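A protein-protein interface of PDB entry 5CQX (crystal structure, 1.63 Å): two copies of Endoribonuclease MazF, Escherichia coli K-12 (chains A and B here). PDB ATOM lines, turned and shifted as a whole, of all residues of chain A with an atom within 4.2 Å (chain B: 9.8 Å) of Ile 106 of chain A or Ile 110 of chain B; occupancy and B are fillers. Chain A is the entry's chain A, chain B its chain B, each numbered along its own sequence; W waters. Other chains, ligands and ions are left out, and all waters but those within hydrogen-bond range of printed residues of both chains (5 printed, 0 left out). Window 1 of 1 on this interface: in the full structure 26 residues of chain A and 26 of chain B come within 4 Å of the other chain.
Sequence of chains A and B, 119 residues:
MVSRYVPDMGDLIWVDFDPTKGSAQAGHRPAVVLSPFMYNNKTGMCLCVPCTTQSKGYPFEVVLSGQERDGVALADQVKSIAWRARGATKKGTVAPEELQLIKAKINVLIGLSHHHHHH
Of the printed residues of chain B, Ile 106 of chain A touches Ile 110.
Ala 104 of chain A touches three residues of chain B.
Leu 109 of chain A touches just these residues of chain B: Leu 34, Ser 35, Pro 36, Tyr 39 and Leu 47.
Of the printed residues of chain A, Lys 103 of chain B touches Ile 110.
Of the printed residues of chain A, Lys 79 of chain B touches Val 78 (3.9 Å).
Of the printed residues of chain A, His 117 of chain B touches Ala 104 (3.3 Å).
The nearest printed residue of chain A that does not touch Ile 110 of chain B is Leu 34 of chain A (4.04 Å).
The nearest printed residue of chain A that does not touch Tyr 39 of chain B is Ala 75 of chain A (7.0 Å).
Printed residues of chain A that touch a printed residue of chain B: Leu 34, Leu 47, Val 78, Lys 103, Ala 104, Lys 105, Ile 106, Val 108, Leu 109 and Ile 110.
Among the printed residues, 24 pairs touch across the chains.
Among the printed residues, no Asp or Glu carboxylate lies within 4 Å of a Lys or Arg side-chain nitrogen of the other chain.
Water W4 bridges the backbone carbonyl oxygen (O) of Lys 103 of chain B (2.7 Å) and the backbone carbonyl oxygen (O) of Ile 110 of chain A (2.8 Å).
Water W1 lies within hydrogen-bond range of NZ of Lys 103 of chain A and O of Gly 111 of chain B.
The side-chain amino group of Lys 103 of chain A sits at hydrogen-bond distance from the backbone carbonyl oxygen of Gly 111 of chain B, 3.0 Å away.
The side-chain amino group of Lys 105 of chain A sits at hydrogen-bond distance from the backbone carbonyl oxygen of His 119 of chain B, 2.7 Å away.
The backbone carbonyl oxygen of Leu 34 of chain A lies close to the backbone carbonyl oxygen of Leu 109 of chain B (3.2 Å).
Among the printed residues, merely in contact across the chains: Ala 104 of chain A with His 117 of chain B, Ile 110 of chain A with Lys 103 of chain B, Leu 47 of chain A with Ile 110 of chain B, Leu 109 of chain A with Pro 36 of chain B, Leu 109 of chain A with Tyr 39 of chain B, Leu 109 of chain A with Ser 35 of chain B, Ala 104 of chain A with Leu 112 of chain B, Ile 106 of chain A with Ile 110 of chain B, Leu 109 of chain A with Leu 34 of chain B, Ile 110 of chain A with Leu 34 of chain B, Val 108 of chain A with His 119 of chain B, Leu 47 of chain A with Leu 109 of chain B, Val 78 of chain A with Val 78 of chain B, Leu 47 of chain A with Val 78 of chain B, Ala 104 of chain A with His 119 of chain B, Val 78 of chain A with Lys 79 of chain B, Ile 110 of chain A with Ile 106 of chain B, Ile 110 of chain A with Leu 47 of chain B, Leu 47 of chain A with Asp 76 of chain B, Leu 109 of chain A with Leu 47 of chain B and Lys 103 of chain A with Leu 112 of chain B.
Leu 47 of chain A touches Leu 109 of chain B, and with the chains exchanged Leu 109 of chain A touches Leu 47 of chain B.
Leu 47 of chain A touches Ile 110 of chain B, and with the chains exchanged Ile 110 of chain A touches Leu 47 of chain B.
N of Leu 34 of chain A lies within hydrogen-bond range of O of Leu 47 of chain A.
O of Leu 34 of chain B sits at hydrogen-bond distance from NZ of Lys 103 of chain B (3.2 Å).
The backbone carbonyl oxygen of His 117 of chain B sits at hydrogen-bond distance from a ring nitrogen (ND1) of His 119 of chain B.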
ATOM      1  N   LEU A  34     -34.039 -25.795   9.273  1.00  0.00           N
ATOM      2  CA  LEU A  34     -33.399 -24.504   9.052  1.00  0.00           C
ATOM      3  C   LEU A  34     -32.130 -24.585   8.206  1.00  0.00           C
ATOM      4  O   LEU A  34     -31.768 -23.630   7.525  1.00  0.00           O
ATOM      5  CB  LEU A  34     -33.034 -23.879  10.398  1.00  0.00           C
ATOM      6  CG  LEU A  34     -34.156 -23.806  11.428  1.00  0.00           C
ATOM      7  CD1 LEU A  34     -33.596 -23.149  12.672  1.00  0.00           C
ATOM      8  CD2 LEU A  34     -35.357 -23.024  10.895  1.00  0.00           C
ATOM      9  N   LEU A  47     -30.362 -28.944  11.214  1.00  0.00           N
ATOM     10  CA  LEU A  47     -30.737 -28.076  12.323  1.00  0.00           C
ATOM     11  C   LEU A  47     -32.208 -27.765  12.129  1.00  0.00           C
ATOM     12  O   LEU A  47     -32.607 -27.220  11.094  1.00  0.00           O
ATOM     13  CB  LEU A  47     -29.902 -26.799  12.315  1.00  0.00           C
ATOM     14  CG  LEU A  47     -29.755 -26.102  13.660  1.00  0.00           C
ATOM     15  CD1 LEU A  47     -29.061 -27.038  14.649  1.00  0.00           C
ATOM     16  CD2 LEU A  47     -28.980 -24.799  13.496  1.00  0.00           C
ATOM     17  N   VAL A  49     -36.323 -26.944  14.139  1.00  0.00           N
ATOM     18  CA  VAL A  49     -37.102 -26.526  15.314  1.00  0.00           C
ATOM     19  C   VAL A  49     -38.375 -27.350  15.425  1.00  0.00           C
ATOM     20  O   VAL A  49     -39.107 -27.525  14.452  1.00  0.00           O
ATOM     21  CB  VAL A  49     -37.448 -24.997  15.357  1.00  0.00           C
ATOM     22  CG1 VAL A  49     -36.182 -24.150  15.362  1.00  0.00           C
ATOM     23  CG2 VAL A  49     -38.356 -24.584  14.219  1.00  0.00           C
ATOM     24  N   ALA A  75     -39.093 -21.702  18.405  1.00  0.00           N
ATOM     25  CA  ALA A  75     -37.799 -21.294  17.870  1.00  0.00           C
ATOM     26  C   ALA A  75     -36.630 -21.527  18.840  1.00  0.00           C
ATOM     27  O   ALA A  75     -35.536 -21.919  18.421  1.00  0.00           O
ATOM     28  CB  ALA A  75     -37.853 -19.829  17.395  1.00  0.00           C
ATOM     29  N   VAL A  78     -34.417 -25.092  19.138  1.00  0.00           N
ATOM     30  CA  VAL A  78     -33.604 -25.540  18.023  1.00  0.00           C
ATOM     31  C   VAL A  78     -32.721 -26.724  18.436  1.00  0.00           C
ATOM     32  O   VAL A  78     -32.250 -26.804  19.573  1.00  0.00           O
ATOM     33  CB  VAL A  78     -32.786 -24.362  17.440  1.00  0.00           C
ATOM     34  CG1 VAL A  78     -31.948 -23.684  18.528  1.00  0.00           C
ATOM     35  CG2 VAL A  78     -31.928 -24.824  16.264  1.00  0.00           C
ATOM     36  N   ILE A 102     -38.623 -17.479  12.331  1.00  0.00           N
ATOM     37  CA  ILE A 102     -37.991 -18.476  13.181  1.00  0.00           C
ATOM     38  C   ILE A 102     -36.486 -18.184  13.306  1.00  0.00           C
ATOM     39  O   ILE A 102     -35.932 -18.136  14.405  1.00  0.00           O
ATOM     40  CB  ILE A 102     -38.233 -19.901  12.607  1.00  0.00           C
ATOM     41  CG1 ILE A 102     -39.735 -20.228  12.630  1.00  0.00           C
ATOM     42  CG2 ILE A 102     -37.398 -20.943  13.347  1.00  0.00           C
ATOM     43  CD1 ILE A 102     -40.080 -21.596  11.922  1.00  0.00           C
ATOM     44  N   LYS A 103     -35.839 -17.970  12.170  1.00  0.00           N
ATOM     45  CA  LYS A 103     -34.405 -17.748  12.135  1.00  0.00           C
ATOM     46  C   LYS A 103     -34.035 -16.476  12.872  1.00  0.00           C
ATOM     47  O   LYS A 103     -33.022 -16.436  13.569  1.00  0.00           O
ATOM     48  CB  LYS A 103     -33.929 -17.656  10.692  1.00  0.00           C
ATOM     49  CG  LYS A 103     -33.909 -18.987   9.982  1.00  0.00           C
ATOM     50  CD  LYS A 103     -33.405 -18.839   8.564  1.00  0.00           C
ATOM     51  CE  LYS A 103     -33.246 -20.200   7.897  1.00  0.00           C
ATOM     52  NZ  LYS A 103     -32.249 -20.160   6.793  1.00  0.00           N
ATOM     53  N   ALA A 104     -34.854 -15.447  12.705  1.00  0.00           N
ATOM     54  CA  ALA A 104     -34.573 -14.152  13.325  1.00  0.00           C
ATOM     55  C   ALA A 104     -34.637 -14.277  14.837  1.00  0.00           C
ATOM     56  O   ALA A 104     -33.821 -13.684  15.561  1.00  0.00           O
ATOM     57  CB  ALA A 104     -35.547 -13.105  12.838  1.00  0.00           C
ATOM     58  N   LYS A 105     -35.605 -15.044  15.328  1.00  0.00           N
ATOM     59  CA  LYS A 105     -35.741 -15.188  16.775  1.00  0.00           C
ATOM     60  C   LYS A 105     -34.540 -15.940  17.357  1.00  0.00           C
ATOM     61  O   LYS A 105     -34.030 -15.579  18.405  1.00  0.00           O
ATOM     62  CB  LYS A 105     -37.070 -15.835  17.149  1.00  0.00           C
ATOM     63  CG  LYS A 105     -38.276 -14.952  16.848  1.00  0.00           C
ATOM     64  CD  LYS A 105     -39.565 -15.626  17.288  1.00  0.00           C
ATOM     65  CE  LYS A 105     -40.803 -14.842  16.877  1.00  0.00           C
ATOM     66  NZ  LYS A 105     -40.958 -13.628  17.722  1.00  0.00           N
ATOM     67  N   ILE A 106     -34.072 -16.974  16.669  1.00  0.00           N
ATOM     68  CA  ILE A 106     -32.868 -17.677  17.106  1.00  0.00           C
ATOM     69  C   ILE A 106     -31.657 -16.732  17.080  1.00  0.00           C
ATOM     70  O   ILE A 106     -30.831 -16.704  18.004  1.00  0.00           O
ATOM     71  CB  ILE A 106     -32.620 -18.914  16.232  1.00  0.00           C
ATOM     72  CG1 ILE A 106     -33.781 -19.884  16.413  1.00  0.00           C
ATOM     73  CG2 ILE A 106     -31.292 -19.580  16.612  1.00  0.00           C
ATOM     74  CD1 ILE A 106     -33.863 -20.982  15.346  1.00  0.00           C
ATOM     75  N   ASN A 107     -31.579 -15.926  16.033  1.00  0.00           N
ATOM     76  CA  ASN A 107     -30.467 -14.996  15.858  1.00  0.00           C
ATOM     77  C   ASN A 107     -30.340 -14.016  17.023  1.00  0.00           C
ATOM     78  O   ASN A 107     -29.235 -13.652  17.407  1.00  0.00           O
ATOM     79  CB  ASN A 107     -30.629 -14.255  14.534  1.00  0.00           C
ATOM     80  CG  ASN A 107     -29.420 -13.442  14.164  1.00  0.00           C
ATOM     81  OD1 ASN A 107     -28.376 -13.990  13.820  1.00  0.00           O
ATOM     82  ND2 ASN A 107     -29.557 -12.121  14.213  1.00  0.00           N
ATOM     83  N   VAL A 108     -31.467 -13.593  17.584  1.00  0.00           N
ATOM     84  CA  VAL A 108     -31.435 -12.704  18.747  1.00  0.00           C
ATOM     85  C   VAL A 108     -30.651 -13.350  19.881  1.00  0.00           C
ATOM     86  O   VAL A 108     -29.928 -12.673  20.610  1.00  0.00           O
ATOM     87  CB  VAL A 108     -32.850 -12.383  19.268  1.00  0.00           C
ATOM     88  CG1 VAL A 108     -32.778 -11.740  20.641  1.00  0.00           C
ATOM     89  CG2 VAL A 108     -33.610 -11.486  18.285  1.00  0.00           C
ATOM     90  N   LEU A 109     -30.785 -14.663  20.030  1.00  0.00           N
ATOM     91  CA  LEU A 109     -30.151 -15.358  21.145  1.00  0.00           C
ATOM     92  C   LEU A 109     -28.692 -15.748  20.912  1.00  0.00           C
ATOM     93  O   LEU A 109     -27.872 -15.685  21.839  1.00  0.00           O
ATOM     94  CB  LEU A 109     -30.952 -16.616  21.506  1.00  0.00           C
ATOM     95  CG  LEU A 109     -32.360 -16.370  22.041  1.00  0.00           C
ATOM     96  CD1 LEU A 109     -33.058 -17.687  22.293  1.00  0.00           C
ATOM     97  CD2 LEU A 109     -32.311 -15.524  23.311  1.00  0.00           C
ATOM     98  N   ILE A 110     -28.356 -16.174  19.695  1.00  0.00           N
ATOM     99  CA  ILE A 110     -27.033 -16.744  19.484  1.00  0.00           C
ATOM    100  C   ILE A 110     -26.294 -16.236  18.241  1.00  0.00           C
ATOM    101  O   ILE A 110     -25.237 -16.754  17.881  1.00  0.00           O
ATOM    102  CB  ILE A 110     -27.106 -18.275  19.481  1.00  0.00           C
ATOM    103  CG1 ILE A 110     -27.992 -18.745  18.328  1.00  0.00           C
ATOM    104  CG2 ILE A 110     -27.658 -18.764  20.811  1.00  0.00           C
ATOM    105  CD1 ILE A 110     -27.891 -20.227  18.067  1.00  0.00           C
ATOM    106  N   LEU B  34     -24.329 -20.332  24.970  1.00  0.00           N
ATOM    107  CA  LEU B  34     -24.340 -19.364  23.869  1.00  0.00           C
ATOM    108  C   LEU B  34     -25.264 -18.169  24.091  1.00  0.00           C
ATOM    109  O   LEU B  34     -24.992 -17.077  23.604  1.00  0.00           O
ATOM    110  CB  LEU B  34     -24.711 -20.040  22.555  1.00  0.00           C
ATOM    111  CG  LEU B  34     -23.786 -21.194  22.160  1.00  0.00           C
ATOM    112  CD1 LEU B  34     -24.153 -21.742  20.771  1.00  0.00           C
ATOM    113  CD2 LEU B  34     -22.298 -20.797  22.212  1.00  0.00           C
ATOM    114  N   SER B  35     -26.365 -18.386  24.797  1.00  0.00           N
ATOM    115  CA  SER B  35     -27.413 -17.385  24.914  1.00  0.00           C
ATOM    116  C   SER B  35     -27.175 -16.430  26.087  1.00  0.00           C
ATOM    117  O   SER B  35     -26.479 -16.782  27.046  1.00  0.00           O
ATOM    118  CB  SER B  35     -28.791 -18.052  25.036  1.00  0.00           C
ATOM    119  OG  SER B  35     -28.815 -19.050  26.040  1.00  0.00           O
ATOM    120  N   PRO B  36     -27.754 -15.222  26.003  1.00  0.00           N
ATOM    121  CA  PRO B  36     -27.452 -14.203  27.021  1.00  0.00           C
ATOM    122  C   PRO B  36     -28.138 -14.439  28.361  1.00  0.00           C
ATOM    123  O   PRO B  36     -29.209 -15.040  28.443  1.00  0.00           O
ATOM    124  CB  PRO B  36     -27.949 -12.900  26.384  1.00  0.00           C
ATOM    125  CG  PRO B  36     -29.002 -13.316  25.411  1.00  0.00           C
ATOM    126  CD  PRO B  36     -28.674 -14.727  24.963  1.00  0.00           C
ATOM    127  N   TYR B  39     -32.111 -13.728  28.835  1.00  0.00           N
ATOM    128  CA  TYR B  39     -32.934 -14.841  28.396  1.00  0.00           C
ATOM    129  C   TYR B  39     -32.835 -16.037  29.354  1.00  0.00           C
ATOM    130  O   TYR B  39     -33.865 -16.607  29.756  1.00  0.00           O
ATOM    131  CB  TYR B  39     -32.554 -15.261  26.969  1.00  0.00           C
ATOM    132  CG  TYR B  39     -33.166 -16.568  26.563  1.00  0.00           C
ATOM    133  CD1 TYR B  39     -34.430 -16.611  25.981  1.00  0.00           C
ATOM    134  CD2 TYR B  39     -32.488 -17.761  26.775  1.00  0.00           C
ATOM    135  CE1 TYR B  39     -35.003 -17.830  25.614  1.00  0.00           C
ATOM    136  CE2 TYR B  39     -33.053 -18.983  26.416  1.00  0.00           C
ATOM    137  CZ  TYR B  39     -34.307 -19.002  25.837  1.00  0.00           C
ATOM    138  OH  TYR B  39     -34.871 -20.210  25.487  1.00  0.00           O
ATOM    139  N   LEU B  47     -29.343 -21.944  25.523  1.00  0.00           N
ATOM    140  CA  LEU B  47     -28.862 -22.650  24.331  1.00  0.00           C
ATOM    141  C   LEU B  47     -27.370 -22.874  24.501  1.00  0.00           C
ATOM    142  O   LEU B  47     -26.620 -21.930  24.831  1.00  0.00           O
ATOM    143  CB  LEU B  47     -29.150 -21.847  23.053  1.00  0.00           C
ATOM    144  CG  LEU B  47     -30.634 -21.729  22.695  1.00  0.00           C
ATOM    145  CD1 LEU B  47     -30.887 -20.865  21.440  1.00  0.00           C
ATOM    146  CD2 LEU B  47     -31.199 -23.125  22.516  1.00  0.00           C
ATOM    147  N   PHE B  60     -17.227 -28.542  12.287  1.00  0.00           N
ATOM    148  CA  PHE B  60     -17.898 -27.667  13.266  1.00  0.00           C
ATOM    149  C   PHE B  60     -17.229 -27.709  14.649  1.00  0.00           C
ATOM    150  O   PHE B  60     -17.684 -27.048  15.601  1.00  0.00           O
ATOM    151  CB  PHE B  60     -19.389 -27.969  13.351  1.00  0.00           C
ATOM    152  CG  PHE B  60     -20.185 -27.380  12.223  1.00  0.00           C
ATOM    153  CD1 PHE B  60     -20.353 -28.072  11.038  1.00  0.00           C
ATOM    154  CD2 PHE B  60     -20.772 -26.123  12.350  1.00  0.00           C
ATOM    155  CE1 PHE B  60     -21.098 -27.527   9.992  1.00  0.00           C
ATOM    156  CE2 PHE B  60     -21.512 -25.571  11.310  1.00  0.00           C
ATOM    157  CZ  PHE B  60     -21.672 -26.280  10.124  1.00  0.00           C
ATOM    158  N   ALA B  75     -20.001 -27.264  17.463  1.00  0.00           N
ATOM    159  CA  ALA B  75     -20.829 -26.091  17.184  1.00  0.00           C
ATOM    160  C   ALA B  75     -22.156 -26.372  16.459  1.00  0.00           C
ATOM    161  O   ALA B  75     -23.096 -25.595  16.568  1.00  0.00           O
ATOM    162  CB  ALA B  75     -20.017 -25.022  16.453  1.00  0.00           C
ATOM    163  N   ASP B  76     -22.249 -27.475  15.725  1.00  0.00           N
ATOM    164  CA  ASP B  76     -23.504 -27.750  15.046  1.00  0.00           C
ATOM    165  C   ASP B  76     -24.504 -28.485  15.931  1.00  0.00           C
ATOM    166  O   ASP B  76     -25.640 -28.711  15.525  1.00  0.00           O
ATOM    167  CB  ASP B  76     -23.273 -28.498  13.734  1.00  0.00           C
ATOM    168  CG  ASP B  76     -22.528 -29.804  13.916  1.00  0.00           C
ATOM    169  OD1 ASP B  76     -21.882 -30.012  14.970  1.00  0.00           O
ATOM    170  OD2 ASP B  76     -22.575 -30.624  12.972  1.00  0.00           O
ATOM    171  N   VAL B  78     -26.133 -27.600  18.691  1.00  0.00           N
ATOM    172  CA  VAL B  78     -26.801 -26.744  19.666  1.00  0.00           C
ATOM    173  C   VAL B  78     -28.070 -27.404  20.211  1.00  0.00           C
ATOM    174  O   VAL B  78     -28.769 -28.151  19.510  1.00  0.00           O
ATOM    175  CB  VAL B  78     -27.084 -25.330  19.107  1.00  0.00           C
ATOM    176  CG1 VAL B  78     -27.844 -25.421  17.820  1.00  0.00           C
ATOM    177  CG2 VAL B  78     -27.820 -24.469  20.137  1.00  0.00           C
ATOM    178  N   LYS B  79     -28.336 -27.164  21.485  1.00  0.00           N
ATOM    179  CA  LYS B  79     -29.514 -27.714  22.141  1.00  0.00           C
ATOM    180  C   LYS B  79     -29.956 -26.762  23.249  1.00  0.00           C
ATOM    181  O   LYS B  79     -29.128 -26.034  23.809  1.00  0.00           O
ATOM    182  CB  LYS B  79     -29.181 -29.078  22.741  1.00  0.00           C
ATOM    183  CG  LYS B  79     -30.375 -29.809  23.316  1.00  0.00           C
ATOM    184  CD  LYS B  79     -29.985 -31.165  23.880  1.00  0.00           C
ATOM    185  CE  LYS B  79     -29.169 -31.001  25.137  1.00  0.00           C
ATOM    186  NZ  LYS B  79     -28.952 -32.304  25.818  1.00  0.00           N
ATOM    187  N   ILE B 102     -17.644 -20.250  17.478  1.00  0.00           N
ATOM    188  CA  ILE B 102     -18.821 -21.109  17.602  1.00  0.00           C
ATOM    189  C   ILE B 102     -20.056 -20.446  16.971  1.00  0.00           C
ATOM    190  O   ILE B 102     -20.762 -21.065  16.179  1.00  0.00           O
ATOM    191  CB  ILE B 102     -19.115 -21.500  19.071  1.00  0.00           C
ATOM    192  CG1 ILE B 102     -17.986 -22.353  19.652  1.00  0.00           C
ATOM    193  CG2 ILE B 102     -20.459 -22.257  19.172  1.00  0.00           C
ATOM    194  CD1 ILE B 102     -18.015 -22.440  21.199  1.00  0.00           C
ATOM    195  N   LYS B 103     -20.313 -19.183  17.310  1.00  0.00           N
ATOM    196  CA  LYS B 103     -21.473 -18.479  16.764  1.00  0.00           C
ATOM    197  C   LYS B 103     -21.346 -18.247  15.257  1.00  0.00           C
ATOM    198  O   LYS B 103     -22.323 -18.338  14.515  1.00  0.00           O
ATOM    199  CB  LYS B 103     -21.697 -17.162  17.506  1.00  0.00           C
ATOM    200  CG  LYS B 103     -22.110 -17.367  18.934  1.00  0.00           C
ATOM    201  CD  LYS B 103     -22.455 -16.034  19.607  1.00  0.00           C
ATOM    202  CE  LYS B 103     -23.068 -16.317  20.955  1.00  0.00           C
ATOM    203  NZ  LYS B 103     -23.373 -15.087  21.728  1.00  0.00           N
ATOM    204  N   ALA B 104     -20.134 -17.964  14.802  1.00  0.00           N
ATOM    205  CA  ALA B 104     -19.886 -17.757  13.380  1.00  0.00           C
ATOM    206  C   ALA B 104     -20.240 -19.008  12.586  1.00  0.00           C
ATOM    207  O   ALA B 104     -20.842 -18.920  11.511  1.00  0.00           O
ATOM    208  CB  ALA B 104     -18.436 -17.383  13.149  1.00  0.00           C
ATOM    209  N   LYS B 105     -19.859 -20.165  13.116  1.00  0.00           N
ATOM    210  CA  LYS B 105     -20.134 -21.438  12.440  1.00  0.00           C
ATOM    211  C   LYS B 105     -21.622 -21.748  12.438  1.00  0.00           C
ATOM    212  O   LYS B 105     -22.185 -22.130  11.413  1.00  0.00           O
ATOM    213  CB  LYS B 105     -19.329 -22.574  13.057  1.00  0.00           C
ATOM    214  CG  LYS B 105     -17.865 -22.564  12.662  1.00  0.00           C
ATOM    215  CD  LYS B 105     -17.135 -23.784  13.222  1.00  0.00           C
ATOM    216  CE  LYS B 105     -15.695 -23.863  12.732  1.00  0.00           C
ATOM    217  NZ  LYS B 105     -14.838 -22.769  13.250  1.00  0.00           N
ATOM    218  N   ILE B 106     -22.277 -21.561  13.575  1.00  0.00           N
ATOM    219  CA  ILE B 106     -23.712 -21.798  13.642  1.00  0.00           C
ATOM    220  C   ILE B 106     -24.512 -20.965  12.629  1.00  0.00           C
ATOM    221  O   ILE B 106     -25.521 -21.435  12.090  1.00  0.00           O
ATOM    222  CB  ILE B 106     -24.252 -21.569  15.057  1.00  0.00           C
ATOM    223  CG1 ILE B 106     -23.873 -22.755  15.936  1.00  0.00           C
ATOM    224  CG2 ILE B 106     -25.768 -21.394  15.024  1.00  0.00           C
ATOM    225  CD1 ILE B 106     -24.117 -22.523  17.420  1.00  0.00           C
ATOM    226  N   ASN B 107     -24.051 -19.743  12.360  1.00  0.00           N
ATOM    227  CA  ASN B 107     -24.719 -18.855  11.406  1.00  0.00           C
ATOM    228  C   ASN B 107     -24.878 -19.458  10.023  1.00  0.00           C
ATOM    229  O   ASN B 107     -25.826 -19.139   9.306  1.00  0.00           O
ATOM    230  CB  ASN B 107     -23.994 -17.511  11.271  1.00  0.00           C
ATOM    231  CG  ASN B 107     -24.665 -16.599  10.239  1.00  0.00           C
ATOM    232  OD1 ASN B 107     -25.765 -16.093  10.468  1.00  0.00           O
ATOM    233  ND2 ASN B 107     -24.013 -16.406   9.095  1.00  0.00           N
ATOM    234  N   VAL B 108     -23.943 -20.314   9.631  1.00  0.00           N
ATOM    235  CA  VAL B 108     -24.026 -20.959   8.329  1.00  0.00           C
ATOM    236  C   VAL B 108     -25.242 -21.877   8.258  1.00  0.00           C
ATOM    237  O   VAL B 108     -25.812 -22.081   7.192  1.00  0.00           O
ATOM    238  CB  VAL B 108     -22.748 -21.753   8.007  1.00  0.00           C
ATOM    239  CG1 VAL B 108     -22.961 -22.613   6.775  1.00  0.00           C
ATOM    240  CG2 VAL B 108     -21.571 -20.799   7.824  1.00  0.00           C
ATOM    241  N   LEU B 109     -25.639 -22.423   9.407  1.00  0.00           N
ATOM    242  CA  LEU B 109     -26.808 -23.300   9.484  1.00  0.00           C
ATOM    243  C   LEU B 109     -28.122 -22.521   9.627  1.00  0.00           C
ATOM    244  O   LEU B 109     -29.190 -23.034   9.332  1.00  0.00           O
ATOM    245  CB  LEU B 109     -26.656 -24.254  10.664  1.00  0.00           C
ATOM    246  CG  LEU B 109     -25.422 -25.136  10.590  1.00  0.00           C
ATOM    247  CD1 LEU B 109     -25.324 -26.026  11.821  1.00  0.00           C
ATOM    248  CD2 LEU B 109     -25.459 -25.956   9.306  1.00  0.00           C
ATOM    249  N   ILE B 110     -28.039 -21.296  10.126  1.00  0.00           N
ATOM    250  CA  ILE B 110     -29.254 -20.489  10.302  1.00  0.00           C
ATOM    251  C   ILE B 110     -29.134 -19.085   9.709  1.00  0.00           C
ATOM    252  O   ILE B 110     -29.581 -18.124  10.321  1.00  0.00           O
ATOM    253  CB  ILE B 110     -29.587 -20.355  11.800  1.00  0.00           C
ATOM    254  CG1 ILE B 110     -28.473 -19.612  12.534  1.00  0.00           C
ATOM    255  CG2 ILE B 110     -29.816 -21.732  12.419  1.00  0.00           C
ATOM    256  CD1 ILE B 110     -28.764 -19.346  13.999  1.00  0.00           C
ATOM    257  N   GLY B 111     -28.547 -18.980   8.527  1.00  0.00           N
ATOM    258  CA  GLY B 111     -28.380 -17.689   7.885  1.00  0.00           C
ATOM    259  C   GLY B 111     -29.700 -17.152   7.376  1.00  0.00           C
ATOM    260  O   GLY B 111     -30.394 -17.835   6.626  1.00  0.00           O
ATOM    261  N   LEU B 112     -30.050 -15.936   7.783  1.00  0.00           N
ATOM    262  CA  LEU B 112     -31.325 -15.338   7.380  1.00  0.00           C
ATOM    263  C   LEU B 112     -31.186 -14.289   6.276  1.00  0.00           C
ATOM    264  O   LEU B 112     -30.079 -13.984   5.827  1.00  0.00           O
ATOM    265  CB  LEU B 112     -32.051 -14.747   8.582  1.00  0.00           C
ATOM    266  CG  LEU B 112     -31.189 -14.136   9.683  1.00  0.00           C
ATOM    267  CD1 LEU B 112     -30.386 -12.978   9.133  1.00  0.00           C
ATOM    268  CD2 LEU B 112     -32.064 -13.683  10.839  1.00  0.00           C
ATOM    269  N   SER B 113     -32.321 -13.763   5.828  1.00  0.00           N
ATOM    270  CA  SER B 113     -32.325 -12.768   4.776  1.00  0.00           C
ATOM    271  C   SER B 113     -32.051 -11.395   5.356  1.00  0.00           C
ATOM    272  O   SER B 113     -32.381 -11.129   6.511  1.00  0.00           O
ATOM    273  N   HIS B 114     -31.470 -10.537   4.530  1.00  0.00           N
ATOM    274  CA  HIS B 114     -31.015  -9.211   4.908  1.00  0.00           C
ATOM    275  C   HIS B 114     -32.100  -8.151   4.732  1.00  0.00           C
ATOM    276  O   HIS B 114     -32.048  -7.366   3.800  1.00  0.00           O
ATOM    277  CB  HIS B 114     -29.804  -8.847   4.032  1.00  0.00           C
ATOM    278  N   HIS B 117     -37.559  -6.481   9.725  1.00  0.00           N
ATOM    279  CA  HIS B 117     -38.882  -7.040   9.979  1.00  0.00           C
ATOM    280  C   HIS B 117     -39.117  -7.213  11.472  1.00  0.00           C
ATOM    281  O   HIS B 117     -38.186  -7.155  12.279  1.00  0.00           O
ATOM    282  CB  HIS B 117     -39.059  -8.373   9.248  1.00  0.00           C
ATOM    283  CG  HIS B 117     -38.106  -9.434   9.692  1.00  0.00           C
ATOM    284  ND1 HIS B 117     -38.422 -10.363  10.661  1.00  0.00           N
ATOM    285  CD2 HIS B 117     -36.838  -9.708   9.309  1.00  0.00           C
ATOM    286  CE1 HIS B 117     -37.391 -11.163  10.852  1.00  0.00           C
ATOM    287  NE2 HIS B 117     -36.414 -10.785  10.046  1.00  0.00           N
ATOM    288  N   HIS B 119     -39.825  -9.152  14.867  1.00  0.00           N
ATOM    289  CA  HIS B 119     -39.437 -10.446  15.404  1.00  0.00           C
ATOM    290  C   HIS B 119     -39.195 -10.407  16.907  1.00  0.00           C
ATOM    291  O   HIS B 119     -39.336 -11.421  17.576  1.00  0.00           O
ATOM    292  CB  HIS B 119     -38.211 -11.006  14.678  1.00  0.00           C
ATOM    293  CG  HIS B 119     -36.968 -10.187  14.846  1.00  0.00           C
ATOM    294  ND1 HIS B 119     -36.739  -9.026  14.139  1.00  0.00           N
ATOM    295  CD2 HIS B 119     -35.869 -10.381  15.611  1.00  0.00           C
ATOM    296  CE1 HIS B 119     -35.564  -8.530  14.477  1.00  0.00           C
ATOM    297  NE2 HIS B 119     -35.015  -9.333  15.369  1.00  0.00           N
HETATM  298  O   HOH W   1     -33.030 -18.385   4.638  1.00  0.00           O
HETATM  299  O   HOH W   2     -32.612 -11.310  14.600  1.00  0.00           O
HETATM  300  O   HOH W   3     -25.503 -13.682  20.487  1.00  0.00           O
HETATM  301  O   HOH W   4     -24.879 -17.951  15.345  1.00  0.00           O
HETATM  302  O   HOH W   5     -30.033 -21.700   6.362  1.00  0.00           O
